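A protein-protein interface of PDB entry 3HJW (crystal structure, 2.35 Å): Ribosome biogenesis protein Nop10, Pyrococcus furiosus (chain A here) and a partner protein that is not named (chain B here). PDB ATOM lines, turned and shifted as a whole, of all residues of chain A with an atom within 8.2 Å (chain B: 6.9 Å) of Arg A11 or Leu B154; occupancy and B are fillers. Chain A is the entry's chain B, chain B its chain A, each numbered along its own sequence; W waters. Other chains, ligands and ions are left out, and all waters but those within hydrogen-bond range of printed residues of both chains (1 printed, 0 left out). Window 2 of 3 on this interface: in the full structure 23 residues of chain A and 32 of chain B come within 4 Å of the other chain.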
ATOM      1  N   ILE A   3     -14.100   1.550 -24.567  1.00  0.00           N
ATOM      2  CA  ILE A   3     -12.985   0.965 -23.806  1.00  0.00           C
ATOM      3  C   ILE A   3     -12.556  -0.390 -24.380  1.00  0.00           C
ATOM      4  O   ILE A   3     -13.372  -1.294 -24.562  1.00  0.00           O
ATOM      5  CB  ILE A   3     -13.282   0.876 -22.276  1.00  0.00           C
ATOM      6  CG1 ILE A   3     -13.612   2.265 -21.707  1.00  0.00           C
ATOM      7  CG2 ILE A   3     -12.084   0.297 -21.526  1.00  0.00           C
ATOM      8  CD1 ILE A   3     -13.964   2.291 -20.213  1.00  0.00           C
ATOM      9  N   ARG A   4     -11.270  -0.506 -24.684  1.00  0.00           N
ATOM     10  CA  ARG A   4     -10.695  -1.743 -25.214  1.00  0.00           C
ATOM     11  C   ARG A   4      -9.550  -2.180 -24.314  1.00  0.00           C
ATOM     12  O   ARG A   4      -9.064  -1.400 -23.486  1.00  0.00           O
ATOM     13  CB  ARG A   4     -10.190  -1.540 -26.651  1.00  0.00           C
ATOM     14  CG  ARG A   4     -11.230  -0.970 -27.610  1.00  0.00           C
ATOM     15  CD  ARG A   4     -10.690  -0.771 -29.027  1.00  0.00           C
ATOM     16  NE  ARG A   4     -10.470  -2.057 -29.686  1.00  0.00           N
ATOM     17  CZ  ARG A   4     -11.416  -2.755 -30.313  1.00  0.00           C
ATOM     18  NH1 ARG A   4     -12.661  -2.294 -30.373  1.00  0.00           N
ATOM     19  NH2 ARG A   4     -11.116  -3.926 -30.863  1.00  0.00           N
ATOM     20  N   LYS A   5      -9.112  -3.425 -24.469  1.00  0.00           N
ATOM     21  CA  LYS A   5      -7.937  -3.894 -23.739  1.00  0.00           C
ATOM     22  C   LYS A   5      -7.158  -4.951 -24.530  1.00  0.00           C
ATOM     23  O   LYS A   5      -7.779  -5.718 -25.271  1.00  0.00           O
ATOM     24  CB  LYS A   5      -8.312  -4.342 -22.319  1.00  0.00           C
ATOM     25  CG  LYS A   5      -8.931  -5.701 -22.221  1.00  0.00           C
ATOM     26  CD  LYS A   5      -8.944  -6.222 -20.776  1.00  0.00           C
ATOM     27  CE  LYS A   5      -7.562  -6.306 -20.202  1.00  0.00           C
ATOM     28  NZ  LYS A   5      -7.614  -6.806 -18.783  1.00  0.00           N
ATOM     29  N   CYS A   6      -5.820  -4.957 -24.417  1.00  0.00           N
ATOM     30  CA  CYS A   6      -4.989  -5.963 -25.125  1.00  0.00           C
ATOM     31  C   CYS A   6      -5.075  -7.318 -24.415  1.00  0.00           C
ATOM     32  O   CYS A   6      -4.885  -7.410 -23.196  1.00  0.00           O
ATOM     33  CB  CYS A   6      -3.543  -5.480 -25.526  1.00  0.00           C
ATOM     34  SG  CYS A   6      -1.998  -6.524 -25.340  1.00  0.00           S
ATOM     35  N   PRO A   7      -5.423  -8.367 -25.182  1.00  0.00           N
ATOM     36  CA  PRO A   7      -5.487  -9.730 -24.645  1.00  0.00           C
ATOM     37  C   PRO A   7      -4.116 -10.227 -24.182  1.00  0.00           C
ATOM     38  O   PRO A   7      -4.038 -11.189 -23.425  1.00  0.00           O
ATOM     39  CB  PRO A   7      -5.990 -10.549 -25.837  1.00  0.00           C
ATOM     40  CG  PRO A   7      -5.558  -9.727 -27.066  1.00  0.00           C
ATOM     41  CD  PRO A   7      -5.779  -8.317 -26.618  1.00  0.00           C
ATOM     42  N   LYS A   8      -3.052  -9.556 -24.613  1.00  0.00           N
ATOM     43  CA  LYS A   8      -1.694  -9.972 -24.257  1.00  0.00           C
ATOM     44  C   LYS A   8      -1.141  -9.165 -23.073  1.00  0.00           C
ATOM     45  O   LYS A   8      -0.828  -9.746 -22.023  1.00  0.00           O
ATOM     46  CB  LYS A   8      -0.763  -9.870 -25.478  1.00  0.00           C
ATOM     47  CG  LYS A   8       0.596 -10.563 -25.310  1.00  0.00           C
ATOM     48  CD  LYS A   8       0.535 -12.096 -25.614  1.00  0.00           C
ATOM     49  CE  LYS A   8      -0.670 -12.818 -24.955  1.00  0.00           C
ATOM     50  NZ  LYS A   8      -0.528 -14.291 -24.957  1.00  0.00           N
ATOM     51  N   CYS A   9      -1.005  -7.848 -23.286  1.00  0.00           N
ATOM     52  CA  CYS A   9      -0.558  -6.855 -22.293  1.00  0.00           C
ATOM     53  C   CYS A   9      -1.539  -6.813 -21.077  1.00  0.00           C
ATOM     54  O   CYS A   9      -1.101  -6.793 -19.931  1.00  0.00           O
ATOM     55  CB  CYS A   9      -0.261  -5.415 -22.943  1.00  0.00           C
ATOM     56  SG  CYS A   9      -0.867  -4.962 -24.834  1.00  0.00           S
ATOM     57  N   GLY A  10      -2.852  -6.819 -21.329  1.00  0.00           N
ATOM     58  CA  GLY A  10      -3.831  -6.458 -20.295  1.00  0.00           C
ATOM     59  C   GLY A  10      -4.088  -4.948 -20.206  1.00  0.00           C
ATOM     60  O   GLY A  10      -4.891  -4.477 -19.398  1.00  0.00           O
ATOM     61  N   ARG A  11      -3.398  -4.190 -21.044  1.00  0.00           N
ATOM     62  CA  ARG A  11      -3.492  -2.738 -21.077  1.00  0.00           C
ATOM     63  C   ARG A  11      -4.868  -2.232 -21.586  1.00  0.00           C
ATOM     64  O   ARG A  11      -5.405  -2.733 -22.560  1.00  0.00           O
ATOM     65  CB  ARG A  11      -2.331  -2.204 -21.919  1.00  0.00           C
ATOM     66  CG  ARG A  11      -2.518  -0.863 -22.534  1.00  0.00           C
ATOM     67  CD  ARG A  11      -1.965   0.264 -21.677  1.00  0.00           C
ATOM     68  NE  ARG A  11      -2.454   1.509 -22.254  1.00  0.00           N
ATOM     69  CZ  ARG A  11      -2.025   2.728 -21.962  1.00  0.00           C
ATOM     70  NH1 ARG A  11      -1.065   2.928 -21.059  1.00  0.00           N
ATOM     71  NH2 ARG A  11      -2.592   3.755 -22.585  1.00  0.00           N
ATOM     72  N   TYR A  12      -5.437  -1.268 -20.867  1.00  0.00           N
ATOM     73  CA  TYR A  12      -6.655  -0.600 -21.285  1.00  0.00           C
ATOM     74  C   TYR A  12      -6.305   0.552 -22.217  1.00  0.00           C
ATOM     75  O   TYR A  12      -5.367   1.306 -21.960  1.00  0.00           O
ATOM     76  CB  TYR A  12      -7.456  -0.100 -20.077  1.00  0.00           C
ATOM     77  CG  TYR A  12      -8.236  -1.202 -19.419  1.00  0.00           C
ATOM     78  CD1 TYR A  12      -7.731  -1.873 -18.305  1.00  0.00           C
ATOM     79  CD2 TYR A  12      -9.462  -1.609 -19.939  1.00  0.00           C
ATOM     80  CE1 TYR A  12      -8.445  -2.911 -17.709  1.00  0.00           C
ATOM     81  CE2 TYR A  12     -10.176  -2.638 -19.365  1.00  0.00           C
ATOM     82  CZ  TYR A  12      -9.669  -3.281 -18.244  1.00  0.00           C
ATOM     83  OH  TYR A  12     -10.396  -4.301 -17.697  1.00  0.00           O
ATOM     84  N   THR A  13      -7.077   0.684 -23.284  1.00  0.00           N
ATOM     85  CA  THR A  13      -6.778   1.638 -24.344  1.00  0.00           C
ATOM     86  C   THR A  13      -8.055   1.968 -25.124  1.00  0.00           C
ATOM     87  O   THR A  13      -9.050   1.249 -25.028  1.00  0.00           O
ATOM     88  CB  THR A  13      -5.611   1.103 -25.274  1.00  0.00           C
ATOM     89  OG1 THR A  13      -5.417   1.975 -26.387  1.00  0.00           O
ATOM     90  CG2 THR A  13      -5.880  -0.309 -25.791  1.00  0.00           C
ATOM     91  N   LEU A  14      -8.034   3.080 -25.855  1.00  0.00           N
ATOM     92  CA  LEU A  14      -9.077   3.381 -26.848  1.00  0.00           C
ATOM     93  C   LEU A  14      -8.704   2.902 -28.265  1.00  0.00           C
ATOM     94  O   LEU A  14      -9.544   2.892 -29.160  1.00  0.00           O
ATOM     95  CB  LEU A  14      -9.389   4.885 -26.861  1.00  0.00           C
ATOM     96  CG  LEU A  14      -9.791   5.499 -25.511  1.00  0.00           C
ATOM     97  CD1 LEU A  14      -9.784   7.000 -25.577  1.00  0.00           C
ATOM     98  CD2 LEU A  14     -11.153   4.999 -25.050  1.00  0.00           C
ATOM     99  N   LYS A  15      -7.452   2.490 -28.453  1.00  0.00           N
ATOM    100  CA  LYS A  15      -6.914   2.143 -29.773  1.00  0.00           C
ATOM    101  C   LYS A  15      -7.188   0.700 -30.171  1.00  0.00           C
ATOM    102  O   LYS A  15      -7.392  -0.167 -29.310  1.00  0.00           O
ATOM    103  CB  LYS A  15      -5.397   2.359 -29.803  1.00  0.00           C
ATOM    104  CG  LYS A  15      -4.925   3.731 -29.322  1.00  0.00           C
ATOM    105  CD  LYS A  15      -3.415   3.758 -29.286  1.00  0.00           C
ATOM    106  CE  LYS A  15      -2.865   4.760 -28.278  1.00  0.00           C
ATOM    107  NZ  LYS A  15      -3.211   6.142 -28.661  1.00  0.00           N
ATOM    108  N   VAL A  17      -4.854  -1.124 -31.783  1.00  0.00           N
ATOM    109  CA  VAL A  17      -3.625  -1.872 -31.526  1.00  0.00           C
ATOM    110  C   VAL A  17      -2.963  -1.373 -30.230  1.00  0.00           C
ATOM    111  O   VAL A  17      -2.806  -0.160 -30.043  1.00  0.00           O
ATOM    112  CB  VAL A  17      -2.610  -1.872 -32.750  1.00  0.00           C
ATOM    113  CG1 VAL A  17      -3.318  -2.029 -34.086  1.00  0.00           C
ATOM    114  CG2 VAL A  17      -1.808  -0.629 -32.795  1.00  0.00           C
ATOM    115  N   CYS A  18      -2.584  -2.310 -29.350  1.00  0.00           N
ATOM    116  CA  CYS A  18      -1.989  -1.977 -28.045  1.00  0.00           C
ATOM    117  C   CYS A  18      -0.762  -1.098 -28.192  1.00  0.00           C
ATOM    118  O   CYS A  18       0.163  -1.449 -28.909  1.00  0.00           O
ATOM    119  CB  CYS A  18      -1.626  -3.239 -27.236  1.00  0.00           C
ATOM    120  SG  CYS A  18      -1.052  -2.988 -25.480  1.00  0.00           S
ATOM    121  N   PRO A  19      -0.763   0.057 -27.509  1.00  0.00           N
ATOM    122  CA  PRO A  19       0.408   0.927 -27.487  1.00  0.00           C
ATOM    123  C   PRO A  19       1.599   0.305 -26.730  1.00  0.00           C
ATOM    124  O   PRO A  19       2.724   0.771 -26.900  1.00  0.00           O
ATOM    125  CB  PRO A  19      -0.099   2.177 -26.751  1.00  0.00           C
ATOM    126  CG  PRO A  19      -1.220   1.674 -25.890  1.00  0.00           C
ATOM    127  CD  PRO A  19      -1.881   0.613 -26.718  1.00  0.00           C
ATOM    128  N   VAL A  20       1.354  -0.722 -25.909  1.00  0.00           N
ATOM    129  CA  VAL A  20       2.430  -1.424 -25.186  1.00  0.00           C
ATOM    130  C   VAL A  20       2.935  -2.669 -25.946  1.00  0.00           C
ATOM    131  O   VAL A  20       4.037  -2.650 -26.470  1.00  0.00           O
ATOM    132  CB  VAL A  20       2.013  -1.829 -23.724  1.00  0.00           C
ATOM    133  CG1 VAL A  20       3.226  -2.384 -22.937  1.00  0.00           C
ATOM    134  CG2 VAL A  20       1.383  -0.645 -22.968  1.00  0.00           C
ATOM    135  N   CYS A  21       2.120  -3.736 -25.973  1.00  0.00           N
ATOM    136  CA  CYS A  21       2.461  -5.061 -26.561  1.00  0.00           C
ATOM    137  C   CYS A  21       2.502  -4.930 -28.128  1.00  0.00           C
ATOM    138  O   CYS A  21       3.385  -5.487 -28.803  1.00  0.00           O
ATOM    139  CB  CYS A  21       1.510  -6.220 -26.004  1.00  0.00           C
ATOM    140  SG  CYS A  21      -0.245  -5.960 -26.458  1.00  0.00           S
ATOM    141  N   GLY A  22       1.570  -4.163 -28.701  1.00  0.00           N
ATOM    142  CA  GLY A  22       1.414  -4.118 -30.168  1.00  0.00           C
ATOM    143  C   GLY A  22       0.335  -5.045 -30.734  1.00  0.00           C
ATOM    144  O   GLY A  22       0.123  -5.076 -31.943  1.00  0.00           O
ATOM    145  N   THR A  25      -6.415  -5.165 -30.107  1.00  0.00           N
ATOM    146  CA  THR A  25      -7.195  -5.060 -28.884  1.00  0.00           C
ATOM    147  C   THR A  25      -8.630  -5.540 -29.081  1.00  0.00           C
ATOM    148  O   THR A  25      -9.149  -5.555 -30.196  1.00  0.00           O
ATOM    149  CB  THR A  25      -7.215  -3.605 -28.359  1.00  0.00           C
ATOM    150  OG1 THR A  25      -7.901  -2.764 -29.295  1.00  0.00           O
ATOM    151  CG2 THR A  25      -5.792  -3.083 -28.142  1.00  0.00           C
ATOM    152  N   LYS A  26      -9.264  -5.915 -27.978  1.00  0.00           N
ATOM    153  CA  LYS A  26     -10.668  -6.327 -27.960  1.00  0.00           C
ATOM    154  C   LYS A  26     -11.486  -5.413 -27.056  1.00  0.00           C
ATOM    155  O   LYS A  26     -10.931  -4.741 -26.193  1.00  0.00           O
ATOM    156  CB  LYS A  26     -10.766  -7.773 -27.483  1.00  0.00           C
ATOM    157  CG  LYS A  26     -10.134  -8.760 -28.462  1.00  0.00           C
ATOM    158  CD  LYS A  26      -9.765 -10.070 -27.773  1.00  0.00           C
ATOM    159  CE  LYS A  26      -9.232 -11.099 -28.783  1.00  0.00           C
ATOM    160  NZ  LYS A  26      -8.995 -12.434 -28.142  1.00  0.00           N
ATOM    161  N   ALA A  28     -13.524  -4.284 -23.964  1.00  0.00           N
ATOM    162  CA  ALA A  28     -13.249  -4.645 -22.569  1.00  0.00           C
ATOM    163  C   ALA A  28     -14.431  -5.305 -21.859  1.00  0.00           C
ATOM    164  O   ALA A  28     -14.249  -6.139 -20.968  1.00  0.00           O
ATOM    165  CB  ALA A  28     -12.810  -3.424 -21.803  1.00  0.00           C
ATOM    166  N   VAL B 104     -11.521   1.333 -14.141  1.00  0.00           N
ATOM    167  CA  VAL B 104     -11.156   2.063 -15.344  1.00  0.00           C
ATOM    168  C   VAL B 104     -12.370   2.876 -15.813  1.00  0.00           C
ATOM    169  O   VAL B 104     -13.464   2.338 -15.992  1.00  0.00           O
ATOM    170  CB  VAL B 104     -10.679   1.144 -16.480  1.00  0.00           C
ATOM    171  CG1 VAL B 104     -10.027   1.973 -17.587  1.00  0.00           C
ATOM    172  CG2 VAL B 104      -9.664   0.202 -15.973  1.00  0.00           C
ATOM    173  N   ALA B 105     -12.169   4.174 -15.998  1.00  0.00           N
ATOM    174  CA  ALA B 105     -13.253   5.061 -16.412  1.00  0.00           C
ATOM    175  C   ALA B 105     -12.920   5.826 -17.678  1.00  0.00           C
ATOM    176  O   ALA B 105     -11.774   6.139 -17.938  1.00  0.00           O
ATOM    177  CB  ALA B 105     -13.619   6.018 -15.294  1.00  0.00           C
ATOM    178  N   GLU B 152      -4.650   7.283 -12.300  1.00  0.00           N
ATOM    179  CA  GLU B 152      -3.688   7.181 -13.380  1.00  0.00           C
ATOM    180  C   GLU B 152      -4.392   7.414 -14.703  1.00  0.00           C
ATOM    181  O   GLU B 152      -5.256   6.624 -15.095  1.00  0.00           O
ATOM    182  CB  GLU B 152      -2.972   5.818 -13.389  1.00  0.00           C
ATOM    183  CG  GLU B 152      -1.982   5.711 -14.558  1.00  0.00           C
ATOM    184  CD  GLU B 152      -1.352   4.330 -14.747  1.00  0.00           C
ATOM    185  OE1 GLU B 152      -0.474   4.209 -15.634  1.00  0.00           O
ATOM    186  OE2 GLU B 152      -1.726   3.371 -14.036  1.00  0.00           O
ATOM    187  N   VAL B 153      -4.016   8.491 -15.381  1.00  0.00           N
ATOM    188  CA  VAL B 153      -4.473   8.763 -16.737  1.00  0.00           C
ATOM    189  C   VAL B 153      -3.732   7.848 -17.714  1.00  0.00           C
ATOM    190  O   VAL B 153      -2.499   7.802 -17.735  1.00  0.00           O
ATOM    191  CB  VAL B 153      -4.236  10.243 -17.128  1.00  0.00           C
ATOM    192  CG1 VAL B 153      -4.662  10.504 -18.576  1.00  0.00           C
ATOM    193  CG2 VAL B 153      -4.955  11.184 -16.147  1.00  0.00           C
ATOM    194  N   LEU B 154      -4.495   7.113 -18.513  1.00  0.00           N
ATOM    195  CA  LEU B 154      -3.926   6.150 -19.447  1.00  0.00           C
ATOM    196  C   LEU B 154      -3.786   6.754 -20.834  1.00  0.00           C
ATOM    197  O   LEU B 154      -2.766   6.541 -21.500  1.00  0.00           O
ATOM    198  CB  LEU B 154      -4.800   4.892 -19.525  1.00  0.00           C
ATOM    199  CG  LEU B 154      -5.082   4.150 -18.219  1.00  0.00           C
ATOM    200  CD1 LEU B 154      -6.162   3.088 -18.404  1.00  0.00           C
ATOM    201  CD2 LEU B 154      -3.804   3.532 -17.649  1.00  0.00           C
ATOM    202  N   GLU B 155      -4.813   7.493 -21.262  1.00  0.00           N
ATOM    203  CA  GLU B 155      -4.904   8.046 -22.612  1.00  0.00           C
ATOM    204  C   GLU B 155      -5.868   9.229 -22.663  1.00  0.00           C
ATOM    205  O   GLU B 155      -6.946   9.200 -22.079  1.00  0.00           O
ATOM    206  CB  GLU B 155      -5.406   6.991 -23.613  1.00  0.00           C
ATOM    207  CG  GLU B 155      -4.436   5.854 -23.887  1.00  0.00           C
ATOM    208  CD  GLU B 155      -4.923   4.850 -24.931  1.00  0.00           C
ATOM    209  OE1 GLU B 155      -6.023   5.030 -25.506  1.00  0.00           O
ATOM    210  OE2 GLU B 155      -4.175   3.885 -25.190  1.00  0.00           O
ATOM    211  N   ILE B 156      -5.476  10.263 -23.393  1.00  0.00           N
ATOM    212  CA  ILE B 156      -6.383  11.339 -23.736  1.00  0.00           C
ATOM    213  C   ILE B 156      -6.538  11.384 -25.252  1.00  0.00           C
ATOM    214  O   ILE B 156      -5.542  11.422 -25.983  1.00  0.00           O
ATOM    215  CB  ILE B 156      -5.886  12.692 -23.187  1.00  0.00           C
ATOM    216  CG1 ILE B 156      -5.713  12.604 -21.665  1.00  0.00           C
ATOM    217  CG2 ILE B 156      -6.853  13.822 -23.580  1.00  0.00           C
ATOM    218  CD1 ILE B 156      -4.751  13.628 -21.070  1.00  0.00           C
ATOM    219  N   VAL B 161     -11.055  11.180 -21.859  1.00  0.00           N
ATOM    220  CA  VAL B 161      -9.974  10.883 -20.931  1.00  0.00           C
ATOM    221  C   VAL B 161     -10.216   9.503 -20.335  1.00  0.00           C
ATOM    222  O   VAL B 161     -11.235   9.256 -19.682  1.00  0.00           O
ATOM    223  CB  VAL B 161      -9.878  11.943 -19.814  1.00  0.00           C
ATOM    224  CG1 VAL B 161      -8.702  11.649 -18.860  1.00  0.00           C
ATOM    225  CG2 VAL B 161      -9.747  13.339 -20.418  1.00  0.00           C
ATOM    226  N   LEU B 162      -9.280   8.602 -20.590  1.00  0.00           N
ATOM    227  CA  LEU B 162      -9.337   7.261 -20.044  1.00  0.00           C
ATOM    228  C   LEU B 162      -8.410   7.190 -18.849  1.00  0.00           C
ATOM    229  O   LEU B 162      -7.240   7.537 -18.963  1.00  0.00           O
ATOM    230  CB  LEU B 162      -8.908   6.253 -21.102  1.00  0.00           C
ATOM    231  CG  LEU B 162      -8.971   4.787 -20.666  1.00  0.00           C
ATOM    232  CD1 LEU B 162     -10.417   4.369 -20.331  1.00  0.00           C
ATOM    233  CD2 LEU B 162      -8.346   3.907 -21.759  1.00  0.00           C
ATOM    234  N   PHE B 163      -8.922   6.747 -17.703  1.00  0.00           N
ATOM    235  CA  PHE B 163      -8.101   6.675 -16.497  1.00  0.00           C
ATOM    236  C   PHE B 163      -8.455   5.531 -15.559  1.00  0.00           C
ATOM    237  O   PHE B 163      -9.593   5.055 -15.536  1.00  0.00           O
ATOM    238  CB  PHE B 163      -8.112   8.020 -15.738  1.00  0.00           C
ATOM    239  CG  PHE B 163      -9.449   8.389 -15.150  1.00  0.00           C
ATOM    240  CD1 PHE B 163      -9.683   8.240 -13.777  1.00  0.00           C
ATOM    241  CD2 PHE B 163     -10.475   8.905 -15.961  1.00  0.00           C
ATOM    242  CE1 PHE B 163     -10.920   8.588 -13.225  1.00  0.00           C
ATOM    243  CE2 PHE B 163     -11.723   9.257 -15.416  1.00  0.00           C
ATOM    244  CZ  PHE B 163     -11.942   9.103 -14.050  1.00  0.00           C
ATOM    245  N   ARG B 164      -7.457   5.092 -14.791  1.00  0.00           N
ATOM    246  CA  ARG B 164      -7.654   4.147 -13.695  1.00  0.00           C
ATOM    247  C   ARG B 164      -7.753   4.925 -12.401  1.00  0.00           C
ATOM    248  O   ARG B 164      -7.074   5.925 -12.216  1.00  0.00           O
ATOM    249  CB  ARG B 164      -6.476   3.156 -13.585  1.00  0.00           C
ATOM    250  CG  ARG B 164      -6.433   2.049 -14.643  1.00  0.00           C
ATOM    251  CD  ARG B 164      -5.559   0.870 -14.167  1.00  0.00           C
ATOM    252  NE  ARG B 164      -5.443  -0.205 -15.159  1.00  0.00           N
ATOM    253  CZ  ARG B 164      -5.818  -1.478 -14.978  1.00  0.00           C
ATOM    254  NH1 ARG B 164      -6.344  -1.894 -13.835  1.00  0.00           N
ATOM    255  NH2 ARG B 164      -5.641  -2.359 -15.953  1.00  0.00           N
HETATM  256  O   HOH W   1      -3.899  -0.249 -18.081  1.00  0.00           O
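The backbone carbonyl oxygen of Leu B154 sits at hydrogen-bond distance from the guanidinium group of Arg A11, at 3.0 Å.
The side-chain carboxylate of Glu B155 is in salt-bridge range of the guanidinium group of Arg A11 (3.1 Å).
OG1 of Thr A13 is in hydrogen-bond range of OE2 of Glu B155, 2.6 Å away.
OE1 of Glu B155 is in hydrogen-bond range of N of Leu A14.
O of Glu B152 lies within hydrogen-bond range of N of Arg B164, 2.7 Å away.
The backbone NH (N) of Leu B162 sits at hydrogen-bond distance from the backbone carbonyl oxygen (O) of Glu B155 (2.8 Å).
The backbone NH of Arg A4 is in hydrogen-bond range of the backbone carbonyl oxygen of Thr A13 (2.9 Å).
O of Lys A15 sits at hydrogen-bond distance from OG1 of Thr A25, at 2.6 Å.
SG of Cys A6 is disulfide-bonded to SG of Cys A21.
SG of Cys A9 forms a disulfide with SG of Cys A21 (2.0 Å).
CD1 of Tyr A12 touches CG2 of Val B104, 3.7 Å away.
CD1 of Leu B154 touches CB of Tyr A12 (3.8 Å).
Tyr A12 touches Leu B162.
Tyr A12 touches Arg B164 (CD1 to NH2, 3.2 Å).
Thr A13 touches Leu B162.
Glu B155 touches Lys A15 (OE2 to CE, 3.5 Å).
CG of Pro A19 touches OE2 of Glu B155, at 3.8 Å.
Leu B154 touches two residues of chain A.
No residue of chain B comes within 4 Å of Gly A10.
Printed residues of chain A within 4 Å of Arg B164: Tyr A12.
Printed residues of chain A within 4 Å of Glu B155: Arg A11 (3.1 Å), Thr A13 (2.6 Å), Leu A14 (2.8 Å), Lys A15 (3.5 Å) and Pro A19 (3.8 Å).
Of the printed residues of chain A, Leu B162 touches Tyr A12 and Thr A13.
Printed residues of chain A within 4 Å of Val B104: Tyr A12.
Arg A4 touches none of the printed residues of chain B.
Thr A25 touches none of the printed residues of chain B.
Hydrophobic or aromatic side chains of chain A that line the printed part of chain B: Tyr A12, Leu A14 and Pro A19.
Of the 11 printed residues of chain B, 5 touch a printed residue of chain A.
Printed residues of chain B that touch a printed residue of chain A: Val B104, Leu B154, Glu B155, Leu B162 and Arg B164.
Hydrophobic or aromatic side chains of chain B that line the printed part of chain A: Val B104, Leu B154 and Leu B162.
Along chain B the printed residues that touch a printed residue of chain A span positions 104 to 164.
Water W1 bridges the guanidinium group (NE) of Arg B164 (3.3 Å) and the backbone NH (N) of Tyr A12 (3.3 Å).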
